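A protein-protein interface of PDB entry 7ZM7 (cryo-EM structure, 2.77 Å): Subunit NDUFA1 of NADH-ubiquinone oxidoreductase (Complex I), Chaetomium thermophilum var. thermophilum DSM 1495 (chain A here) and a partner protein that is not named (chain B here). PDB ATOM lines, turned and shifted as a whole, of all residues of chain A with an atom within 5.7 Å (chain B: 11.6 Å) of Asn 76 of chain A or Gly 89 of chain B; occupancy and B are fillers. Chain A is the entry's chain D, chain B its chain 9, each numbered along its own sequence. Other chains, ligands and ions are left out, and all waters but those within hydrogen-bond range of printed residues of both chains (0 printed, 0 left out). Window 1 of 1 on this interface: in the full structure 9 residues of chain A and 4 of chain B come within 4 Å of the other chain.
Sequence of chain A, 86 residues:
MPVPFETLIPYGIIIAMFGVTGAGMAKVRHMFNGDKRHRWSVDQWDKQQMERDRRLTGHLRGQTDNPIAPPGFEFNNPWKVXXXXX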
ATOM      1  N   ARG A  55     -27.501  11.273  25.304  1.00  0.00           N
ATOM      2  CA  ARG A  55     -26.109  11.168  25.703  1.00  0.00           C
ATOM      3  C   ARG A  55     -25.559   9.779  25.440  1.00  0.00           C
ATOM      4  O   ARG A  55     -24.408   9.631  25.027  1.00  0.00           O
ATOM      5  CB  ARG A  55     -25.961  11.523  27.176  1.00  0.00           C
ATOM      6  CG  ARG A  55     -25.920  12.985  27.441  1.00  0.00           C
ATOM      7  CD  ARG A  55     -25.884  13.254  28.905  1.00  0.00           C
ATOM      8  NE  ARG A  55     -24.575  12.976  29.455  1.00  0.00           N
ATOM      9  CZ  ARG A  55     -24.364  12.404  30.629  1.00  0.00           C
ATOM     10  NH1 ARG A  55     -25.385  12.035  31.377  1.00  0.00           N
ATOM     11  NH2 ARG A  55     -23.129  12.194  31.049  1.00  0.00           N
ATOM     12  N   LEU A  56     -26.353   8.748  25.694  1.00  0.00           N
ATOM     13  CA  LEU A  56     -25.848   7.394  25.524  1.00  0.00           C
ATOM     14  C   LEU A  56     -25.912   6.938  24.074  1.00  0.00           C
ATOM     15  O   LEU A  56     -25.013   6.237  23.610  1.00  0.00           O
ATOM     16  CB  LEU A  56     -26.614   6.432  26.427  1.00  0.00           C
ATOM     17  CG  LEU A  56     -26.253   6.543  27.899  1.00  0.00           C
ATOM     18  CD1 LEU A  56     -27.332   5.943  28.760  1.00  0.00           C
ATOM     19  CD2 LEU A  56     -24.933   5.890  28.174  1.00  0.00           C
ATOM     20  N   PRO A  70     -20.407   4.025  27.685  1.00  0.00           N
ATOM     21  CA  PRO A  70     -19.236   4.027  26.804  1.00  0.00           C
ATOM     22  C   PRO A  70     -18.293   5.172  27.127  1.00  0.00           C
ATOM     23  O   PRO A  70     -18.710   6.188  27.701  1.00  0.00           O
ATOM     24  CB  PRO A  70     -19.850   4.187  25.409  1.00  0.00           C
ATOM     25  CG  PRO A  70     -21.151   4.833  25.652  1.00  0.00           C
ATOM     26  CD  PRO A  70     -21.639   4.395  26.977  1.00  0.00           C
ATOM     27  N   PRO A  71     -17.013   5.044  26.774  1.00  0.00           N
ATOM     28  CA  PRO A  71     -16.042   6.094  27.111  1.00  0.00           C
ATOM     29  C   PRO A  71     -16.386   7.421  26.456  1.00  0.00           C
ATOM     30  O   PRO A  71     -16.772   7.482  25.288  1.00  0.00           O
ATOM     31  CB  PRO A  71     -14.718   5.533  26.586  1.00  0.00           C
ATOM     32  CG  PRO A  71     -15.110   4.538  25.560  1.00  0.00           C
ATOM     33  CD  PRO A  71     -16.384   3.931  26.048  1.00  0.00           C
ATOM     34  N   GLY A  72     -16.199   8.493  27.213  1.00  0.00           N
ATOM     35  CA  GLY A  72     -16.670   9.798  26.824  1.00  0.00           C
ATOM     36  C   GLY A  72     -17.999  10.193  27.426  1.00  0.00           C
ATOM     37  O   GLY A  72     -18.300  11.385  27.482  1.00  0.00           O
ATOM     38  N   PHE A  73     -18.799   9.235  27.903  1.00  0.00           N
ATOM     39  CA  PHE A  73     -20.142   9.538  28.471  1.00  0.00           C
ATOM     40  C   PHE A  73     -20.025  10.585  29.580  1.00  0.00           C
ATOM     41  O   PHE A  73     -20.899  11.449  29.698  1.00  0.00           O
ATOM     42  CB  PHE A  73     -20.786   8.282  29.060  1.00  0.00           C
ATOM     43  CG  PHE A  73     -22.124   8.508  29.715  1.00  0.00           C
ATOM     44  CD1 PHE A  73     -23.214   8.922  28.970  1.00  0.00           C
ATOM     45  CD2 PHE A  73     -22.289   8.319  31.076  1.00  0.00           C
ATOM     46  CE1 PHE A  73     -24.440   9.139  29.573  1.00  0.00           C
ATOM     47  CE2 PHE A  73     -23.520   8.525  31.675  1.00  0.00           C
ATOM     48  CZ  PHE A  73     -24.594   8.934  30.922  1.00  0.00           C
ATOM     49  N   GLU A  74     -18.943  10.530  30.355  1.00  0.00           N
ATOM     50  CA  GLU A  74     -18.753  11.459  31.493  1.00  0.00           C
ATOM     51  C   GLU A  74     -18.738  12.933  31.034  1.00  0.00           C
ATOM     52  O   GLU A  74     -19.178  13.778  31.827  1.00  0.00           O
ATOM     53  CB  GLU A  74     -17.467  11.059  32.202  1.00  0.00           C
ATOM     54  CG  GLU A  74     -16.348  10.667  31.254  1.00  0.00           C
ATOM     55  CD  GLU A  74     -16.136   9.175  31.060  1.00  0.00           C
ATOM     56  OE1 GLU A  74     -16.979   8.535  30.400  1.00  0.00           O
ATOM     57  OE2 GLU A  74     -15.128   8.654  31.573  1.00  0.00           O
ATOM     58  N   PHE A  75     -18.219  13.248  29.844  1.00  0.00           N
ATOM     59  CA  PHE A  75     -18.080  14.655  29.385  1.00  0.00           C
ATOM     60  C   PHE A  75     -19.207  15.134  28.455  1.00  0.00           C
ATOM     61  O   PHE A  75     -19.179  16.321  28.113  1.00  0.00           O
ATOM     62  CB  PHE A  75     -16.782  14.789  28.583  1.00  0.00           C
ATOM     63  CG  PHE A  75     -15.574  14.181  29.246  1.00  0.00           C
ATOM     64  CD1 PHE A  75     -15.022  14.761  30.374  1.00  0.00           C
ATOM     65  CD2 PHE A  75     -14.992  13.031  28.739  1.00  0.00           C
ATOM     66  CE1 PHE A  75     -13.916  14.199  30.987  1.00  0.00           C
ATOM     67  CE2 PHE A  75     -13.884  12.472  29.355  1.00  0.00           C
ATOM     68  CZ  PHE A  75     -13.350  13.056  30.477  1.00  0.00           C
ATOM     69  N   ASN A  76     -20.160  14.283  28.066  1.00  0.00           N
ATOM     70  CA  ASN A  76     -21.196  14.674  27.071  1.00  0.00           C
ATOM     71  C   ASN A  76     -22.432  15.243  27.763  1.00  0.00           C
ATOM     72  O   ASN A  76     -23.396  15.552  27.051  1.00  0.00           O
ATOM     73  CB  ASN A  76     -21.508  13.565  26.065  1.00  0.00           C
ATOM     74  CG  ASN A  76     -22.058  12.283  26.645  1.00  0.00           C
ATOM     75  OD1 ASN A  76     -22.571  12.260  27.756  1.00  0.00           O
ATOM     76  ND2 ASN A  76     -21.982  11.209  25.880  1.00  0.00           N
ATOM     77  N   ASN A  77     -22.386  15.387  29.087  1.00  0.00           N
ATOM     78  CA  ASN A  77     -23.517  15.934  29.883  1.00  0.00           C
ATOM     79  C   ASN A  77     -23.766  17.349  29.384  1.00  0.00           C
ATOM     80  O   ASN A  77     -22.860  18.178  29.533  1.00  0.00           O
ATOM     81  CB  ASN A  77     -23.246  15.869  31.386  1.00  0.00           C
ATOM     82  CG  ASN A  77     -24.434  16.307  32.214  1.00  0.00           C
ATOM     83  OD1 ASN A  77     -25.577  16.056  31.846  1.00  0.00           O
ATOM     84  ND2 ASN A  77     -24.175  16.958  33.334  1.00  0.00           N
ATOM     85  N   PRO A  78     -24.951  17.684  28.849  1.00  0.00           N
ATOM     86  CA  PRO A  78     -25.161  18.993  28.239  1.00  0.00           C
ATOM     87  C   PRO A  78     -25.571  20.084  29.230  1.00  0.00           C
ATOM     88  O   PRO A  78     -26.554  19.919  29.908  1.00  0.00           O
ATOM     89  CB  PRO A  78     -26.279  18.706  27.234  1.00  0.00           C
ATOM     90  CG  PRO A  78     -27.053  17.530  27.807  1.00  0.00           C
ATOM     91  CD  PRO A  78     -26.141  16.839  28.801  1.00  0.00           C
ATOM     92  N   THR B  81     -15.484  19.868  14.790  1.00  0.00           N
ATOM     93  CA  THR B  81     -16.755  20.361  14.293  1.00  0.00           C
ATOM     94  C   THR B  81     -17.873  19.962  15.244  1.00  0.00           C
ATOM     95  O   THR B  81     -17.699  19.113  16.119  1.00  0.00           O
ATOM     96  CB  THR B  81     -17.043  19.831  12.891  1.00  0.00           C
ATOM     97  OG1 THR B  81     -18.090  20.609  12.299  1.00  0.00           O
ATOM     98  CG2 THR B  81     -17.483  18.383  12.949  1.00  0.00           C
ATOM     99  N   ALA B  82     -19.026  20.605  15.079  1.00  0.00           N
ATOM    100  CA  ALA B  82     -20.141  20.316  15.970  1.00  0.00           C
ATOM    101  C   ALA B  82     -20.579  18.868  15.834  1.00  0.00           C
ATOM    102  O   ALA B  82     -20.861  18.201  16.835  1.00  0.00           O
ATOM    103  CB  ALA B  82     -21.308  21.265  15.693  1.00  0.00           C
ATOM    104  N   GLY B  83     -20.617  18.358  14.602  1.00  0.00           N
ATOM    105  CA  GLY B  83     -21.006  16.976  14.398  1.00  0.00           C
ATOM    106  C   GLY B  83     -20.104  16.004  15.131  1.00  0.00           C
ATOM    107  O   GLY B  83     -20.555  14.960  15.603  1.00  0.00           O
ATOM    108  N   GLN B  84     -18.814  16.326  15.224  1.00  0.00           N
ATOM    109  CA  GLN B  84     -17.902  15.487  15.989  1.00  0.00           C
ATOM    110  C   GLN B  84     -18.210  15.543  17.478  1.00  0.00           C
ATOM    111  O   GLN B  84     -18.264  14.503  18.140  1.00  0.00           O
ATOM    112  CB  GLN B  84     -16.463  15.902  15.710  1.00  0.00           C
ATOM    113  CG  GLN B  84     -15.980  15.496  14.341  1.00  0.00           C
ATOM    114  CD  GLN B  84     -14.625  16.077  14.005  1.00  0.00           C
ATOM    115  OE1 GLN B  84     -14.421  17.288  14.085  1.00  0.00           O
ATOM    116  NE2 GLN B  84     -13.694  15.219  13.609  1.00  0.00           N
ATOM    117  N   ILE B  85     -18.444  16.739  18.018  1.00  0.00           N
ATOM    118  CA  ILE B  85     -18.819  16.860  19.425  1.00  0.00           C
ATOM    119  C   ILE B  85     -20.128  16.136  19.697  1.00  0.00           C
ATOM    120  O   ILE B  85     -20.305  15.523  20.751  1.00  0.00           O
ATOM    121  CB  ILE B  85     -18.921  18.338  19.834  1.00  0.00           C
ATOM    122  CG1 ILE B  85     -17.723  19.135  19.330  1.00  0.00           C
ATOM    123  CG2 ILE B  85     -19.033  18.458  21.335  1.00  0.00           C
ATOM    124  CD1 ILE B  85     -17.918  20.598  19.478  1.00  0.00           C
ATOM    125  N   ARG B  86     -21.067  16.203  18.760  1.00  0.00           N
ATOM    126  CA  ARG B  86     -22.353  15.559  18.953  1.00  0.00           C
ATOM    127  C   ARG B  86     -22.268  14.044  18.901  1.00  0.00           C
ATOM    128  O   ARG B  86     -23.243  13.373  19.245  1.00  0.00           O
ATOM    129  CB  ARG B  86     -23.356  16.078  17.924  1.00  0.00           C
ATOM    130  CG  ARG B  86     -24.294  17.110  18.518  1.00  0.00           C
ATOM    131  CD  ARG B  86     -25.379  17.543  17.569  1.00  0.00           C
ATOM    132  NE  ARG B  86     -24.935  18.554  16.620  1.00  0.00           N
ATOM    133  CZ  ARG B  86     -25.224  19.846  16.717  1.00  0.00           C
ATOM    134  NH1 ARG B  86     -25.943  20.296  17.725  1.00  0.00           N
ATOM    135  NH2 ARG B  86     -24.788  20.692  15.803  1.00  0.00           N
ATOM    136  N   ASN B  87     -21.148  13.480  18.477  1.00  0.00           N
ATOM    137  CA  ASN B  87     -20.973  12.038  18.553  1.00  0.00           C
ATOM    138  C   ASN B  87     -20.139  11.608  19.748  1.00  0.00           C
ATOM    139  O   ASN B  87     -19.844  10.422  19.878  1.00  0.00           O
ATOM    140  CB  ASN B  87     -20.344  11.513  17.266  1.00  0.00           C
ATOM    141  CG  ASN B  87     -21.248  11.665  16.078  1.00  0.00           C
ATOM    142  OD1 ASN B  87     -22.173  12.474  16.090  1.00  0.00           O
ATOM    143  ND2 ASN B  87     -20.982  10.894  15.030  1.00  0.00           N
ATOM    144  N   LEU B  88     -19.767  12.539  20.618  1.00  0.00           N
ATOM    145  CA  LEU B  88     -18.916  12.225  21.755  1.00  0.00           C
ATOM    146  C   LEU B  88     -19.592  11.204  22.657  1.00  0.00           C
ATOM    147  O   LEU B  88     -20.799  11.260  22.884  1.00  0.00           O
ATOM    148  CB  LEU B  88     -18.612  13.501  22.537  1.00  0.00           C
ATOM    149  CG  LEU B  88     -17.595  13.475  23.676  1.00  0.00           C
ATOM    150  CD1 LEU B  88     -16.989  14.841  23.854  1.00  0.00           C
ATOM    151  CD2 LEU B  88     -18.189  13.026  24.977  1.00  0.00           C
ATOM    152  N   GLY B  89     -18.804  10.273  23.178  1.00  0.00           N
ATOM    153  CA  GLY B  89     -19.289   9.307  24.137  1.00  0.00           C
ATOM    154  C   GLY B  89     -20.280   8.318  23.597  1.00  0.00           C
ATOM    155  O   GLY B  89     -20.901   7.599  24.376  1.00  0.00           O
ATOM    156  N   LEU B  90     -20.454   8.262  22.287  1.00  0.00           N
ATOM    157  CA  LEU B  90     -21.402   7.358  21.671  1.00  0.00           C
ATOM    158  C   LEU B  90     -20.706   6.056  21.310  1.00  0.00           C
ATOM    159  O   LEU B  90     -19.567   6.048  20.838  1.00  0.00           O
ATOM    160  CB  LEU B  90     -22.024   8.010  20.438  1.00  0.00           C
ATOM    161  CG  LEU B  90     -23.399   8.630  20.644  1.00  0.00           C
ATOM    162  CD1 LEU B  90     -23.415   9.608  21.784  1.00  0.00           C
ATOM    163  CD2 LEU B  90     -23.831   9.305  19.388  1.00  0.00           C
ATOM    164  N   LEU B  91     -21.423   4.949  21.520  1.00  0.00           N
ATOM    165  CA  LEU B  91     -20.830   3.618  21.564  1.00  0.00           C
ATOM    166  C   LEU B  91     -20.277   3.144  20.228  1.00  0.00           C
ATOM    167  O   LEU B  91     -19.590   2.119  20.198  1.00  0.00           O
ATOM    168  CB  LEU B  91     -21.853   2.599  22.072  1.00  0.00           C
ATOM    169  CG  LEU B  91     -23.004   2.182  21.153  1.00  0.00           C
ATOM    170  CD1 LEU B  91     -23.655   0.920  21.690  1.00  0.00           C
ATOM    171  CD2 LEU B  91     -24.044   3.280  21.021  1.00  0.00           C
ATOM    172  N   ASN B  92     -20.563   3.835  19.128  1.00  0.00           N
ATOM    173  CA  ASN B  92     -20.040   3.420  17.833  1.00  0.00           C
ATOM    174  C   ASN B  92     -19.223   4.511  17.155  1.00  0.00           C
ATOM    175  O   ASN B  92     -18.937   4.399  15.958  1.00  0.00           O
ATOM    176  CB  ASN B  92     -21.179   2.971  16.914  1.00  0.00           C
ATOM    177  CG  ASN B  92     -20.733   1.939  15.902  1.00  0.00           C
ATOM    178  OD1 ASN B  92     -19.579   1.514  15.901  1.00  0.00           O
ATOM    179  ND2 ASN B  92     -21.649   1.529  15.032  1.00  0.00           N
ATOM    180  N   LYS B  93     -18.828   5.551  17.885  1.00  0.00           N
ATOM    181  CA  LYS B  93     -18.080   6.657  17.302  1.00  0.00           C
ATOM    182  C   LYS B  93     -16.801   6.917  18.088  1.00  0.00           C
ATOM    183  O   LYS B  93     -16.506   8.063  18.439  1.00  0.00           O
ATOM    184  CB  LYS B  93     -18.942   7.921  17.260  1.00  0.00           C
ATOM    185  CG  LYS B  93     -20.221   7.774  16.457  1.00  0.00           C
ATOM    186  CD  LYS B  93     -19.927   7.326  15.039  1.00  0.00           C
ATOM    187  CE  LYS B  93     -21.130   7.529  14.142  1.00  0.00           C
ATOM    188  NZ  LYS B  93     -22.402   7.413  14.903  1.00  0.00           N
ATOM    189  N   GLU B  94     -16.040   5.857  18.376  1.00  0.00           N
ATOM    190  CA  GLU B  94     -14.833   6.012  19.183  1.00  0.00           C
ATOM    191  C   GLU B  94     -13.826   6.943  18.526  1.00  0.00           C
ATOM    192  O   GLU B  94     -13.069   7.625  19.224  1.00  0.00           O
ATOM    193  CB  GLU B  94     -14.195   4.651  19.447  1.00  0.00           C
ATOM    194  CG  GLU B  94     -14.909   3.833  20.503  1.00  0.00           C
ATOM    195  CD  GLU B  94     -16.132   3.127  19.962  1.00  0.00           C
ATOM    196  OE1 GLU B  94     -16.372   3.199  18.739  1.00  0.00           O
ATOM    197  OE2 GLU B  94     -16.856   2.499  20.763  1.00  0.00           O
ATOM    198  N   GLU B  95     -13.799   6.987  17.194  1.00  0.00           N
ATOM    199  CA  GLU B  95     -12.845   7.850  16.509  1.00  0.00           C
ATOM    200  C   GLU B  95     -13.088   9.314  16.841  1.00  0.00           C
ATOM    201  O   GLU B  95     -12.140  10.066  17.092  1.00  0.00           O
ATOM    202  CB  GLU B  95     -12.922   7.624  15.001  1.00  0.00           C
ATOM    203  CG  GLU B  95     -12.549   6.220  14.575  1.00  0.00           C
ATOM    204  CD  GLU B  95     -11.107   5.884  14.888  1.00  0.00           C
ATOM    205  OE1 GLU B  95     -10.260   6.799  14.852  1.00  0.00           O
ATOM    206  OE2 GLU B  95     -10.822   4.702  15.173  1.00  0.00           O
ATOM    207  N   ASP B  96     -14.354   9.738  16.853  1.00  0.00           N
ATOM    208  CA  ASP B  96     -14.656  11.139  17.127  1.00  0.00           C
ATOM    209  C   ASP B  96     -14.321  11.527  18.559  1.00  0.00           C
ATOM    210  O   ASP B  96     -13.824  12.631  18.793  1.00  0.00           O
ATOM    211  CB  ASP B  96     -16.122  11.437  16.828  1.00  0.00           C
ATOM    212  CG  ASP B  96     -16.363  11.753  15.367  1.00  0.00           C
ATOM    213  OD1 ASP B  96     -15.413  12.207  14.696  1.00  0.00           O
ATOM    214  OD2 ASP B  96     -17.500  11.554  14.893  1.00  0.00           O
ATOM    215  N   THR B  97     -14.581  10.645  19.524  1.00  0.00           N
ATOM    216  CA  THR B  97     -14.279  10.974  20.909  1.00  0.00           C
ATOM    217  C   THR B  97     -12.786  11.141  21.134  1.00  0.00           C
ATOM    218  O   THR B  97     -12.373  12.024  21.890  1.00  0.00           O
ATOM    219  CB  THR B  97     -14.828   9.903  21.843  1.00  0.00           C
ATOM    220  OG1 THR B  97     -14.050   8.709  21.704  1.00  0.00           O
ATOM    221  CG2 THR B  97     -16.250   9.600  21.494  1.00  0.00           C
ATOM    222  N   LYS B  98     -11.962  10.305  20.508  1.00  0.00           N
ATOM    223  CA  LYS B  98     -10.523  10.480  20.653  1.00  0.00           C
ATOM    224  C   LYS B  98     -10.068  11.814  20.082  1.00  0.00           C
ATOM    225  O   LYS B  98      -9.185  12.465  20.649  1.00  0.00           O
ATOM    226  CB  LYS B  98      -9.773   9.329  19.988  1.00  0.00           C
ATOM    227  CG  LYS B  98      -9.404   8.211  20.946  1.00  0.00           C
ATOM    228  CD  LYS B  98      -8.691   7.080  20.228  1.00  0.00           C
ATOM    229  CE  LYS B  98      -8.881   5.759  20.954  1.00  0.00           C
ATOM    230  NZ  LYS B  98      -7.942   4.715  20.460  1.00  0.00           N
ATOM    231  N   LYS B  99     -10.657  12.237  18.963  1.00  0.00           N
ATOM    232  CA  LYS B  99     -10.312  13.538  18.404  1.00  0.00           C
ATOM    233  C   LYS B  99     -10.716  14.667  19.342  1.00  0.00           C
ATOM    234  O   LYS B  99      -9.984  15.651  19.487  1.00  0.00           O
ATOM    235  CB  LYS B  99     -10.966  13.716  17.039  1.00  0.00           C
ATOM    236  CG  LYS B  99     -10.654  15.043  16.382  1.00  0.00           C
ATOM    237  CD  LYS B  99      -9.156  15.235  16.239  1.00  0.00           C
ATOM    238  CE  LYS B  99      -8.555  14.236  15.266  1.00  0.00           C
ATOM    239  NZ  LYS B  99      -7.085  14.425  15.131  1.00  0.00           N
ATOM    240  N   VAL B 100     -11.880  14.549  19.980  1.00  0.00           N
ATOM    241  CA  VAL B 100     -12.340  15.619  20.854  1.00  0.00           C
ATOM    242  C   VAL B 100     -11.424  15.759  22.062  1.00  0.00           C
ATOM    243  O   VAL B 100     -11.064  16.872  22.463  1.00  0.00           O
ATOM    244  CB  VAL B 100     -13.795  15.377  21.274  1.00  0.00           C
ATOM    245  CG1 VAL B 100     -14.222  16.428  22.269  1.00  0.00           C
ATOM    246  CG2 VAL B 100     -14.703  15.410  20.068  1.00  0.00           C
ATOM    247  N   HIS B 101     -11.031  14.629  22.659  1.00  0.00           N
ATOM    248  CA  HIS B 101     -10.236  14.680  23.917  1.00  0.00           C
ATOM    249  C   HIS B 101      -8.727  14.714  23.650  1.00  0.00           C
ATOM    250  O   HIS B 101      -7.972  14.718  24.644  1.00  0.00           O
ATOM    251  CB  HIS B 101     -10.634  13.521  24.838  1.00  0.00           C
ATOM    252  CG  HIS B 101     -12.103  13.455  25.084  1.00  0.00           C
ATOM    253  ND1 HIS B 101     -12.810  14.526  25.588  1.00  0.00           N
ATOM    254  CD2 HIS B 101     -12.996  12.460  24.901  1.00  0.00           C
ATOM    255  CE1 HIS B 101     -14.079  14.195  25.701  1.00  0.00           C
ATOM    256  NE2 HIS B 101     -14.219  12.931  25.287  1.00  0.00           N
ATOM    257  N   CYS B 102      -8.307  14.727  22.383  1.00  0.00           N
ATOM    258  CA  CYS B 102      -6.889  14.826  22.040  1.00  0.00           C
ATOM    259  C   CYS B 102      -6.057  13.820  22.829  1.00  0.00           C
ATOM    260  O   CYS B 102      -4.979  14.131  23.339  1.00  0.00           O
ATOM    261  CB  CYS B 102      -6.372  16.250  22.247  1.00  0.00           C
ATOM    262  SG  CYS B 102      -7.141  17.477  21.167  1.00  0.00           S
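Arg 55 of chain A touches Leu 90 of chain B (O to CD1, 3.4 Å).
O of Gly 89 of chain B touches CG of Pro 70 of chain A (3.1 Å).
O of Pro 71 of chain A touches CA of Gly 89 of chain B, at 3.3 Å.
Gly 72 of chain A touches Leu 88 of chain B (O to CD2, 3.0 Å).
Gly 89 of chain B touches Gly 72 of chain A.
Phe 73 of chain A touches Gly 89 of chain B.
CE1 of His 101 of chain B touches CD2 of Phe 75 of chain A (3.4 Å).
CA of Gly 89 of chain B touches ND2 of Asn 76 of chain A (3.7 Å).
The guanidinium group (NH2) of Arg 55 of chain A sits at hydrogen-bond distance from the backbone carbonyl oxygen (O) of Phe 73 of chain A (2.7 Å).
The guanidinium group (NE) of Arg 55 of chain A lies within hydrogen-bond range of the side-chain amide oxygen (OD1) of Asn 76 of chain A.
The side-chain carboxylate (OE1) of Glu 74 of chain A lies within hydrogen-bond range of the backbone NH (N) of Gly 72 of chain A.
The backbone carbonyl oxygen (O) of Phe 73 of chain A sits close to the side-chain amide oxygen (OD1) of Asn 76 of chain A (2.7 Å).
The side-chain amide nitrogen of Asn 76 of chain A is in hydrogen-bond range of the backbone carbonyl oxygen of Leu 88 of chain B (3.2 Å).
Asn 76 of chain A touches two residues of chain B.
Gly 89 of chain B touches just these residues of chain A: Pro 70, Pro 71, Gly 72, Phe 73 and Asn 76.
Of chain B, only Leu 90 (3.4 Å) comes within 4 Å of Arg 55 of chain A.
Pro 71 of chain A touches just one residue of chain B: Gly 89 (3.3 Å).
No residue of chain B comes within 4 Å of Asn 77 of chain A.
Pro 78 of chain A touches none of the printed residues of chain B.
Printed residues of chain A within 4 Å of His 101 of chain B: Phe 75 (3.4 Å).
Of the printed residues of chain A, Leu 90 of chain B touches Arg 55 (3.4 Å).
Printed residues of chain B within 4 Å of Pro 70 of chain A: Gly 89 (3.1 Å).
Printed residues of chain A within 4 Å of Leu 88 of chain B: Gly 72 and Asn 76.
Glu 94 of chain B touches none of the printed residues of chain A.
Printed residues of chain A that touch a printed residue of chain B: Arg 55, Pro 70, Pro 71, Gly 72, Phe 73, Phe 75 and Asn 76.
Among the printed residues, no Asp or Glu carboxylate lies within 4 Å of a Lys or Arg side-chain nitrogen of the other chain.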
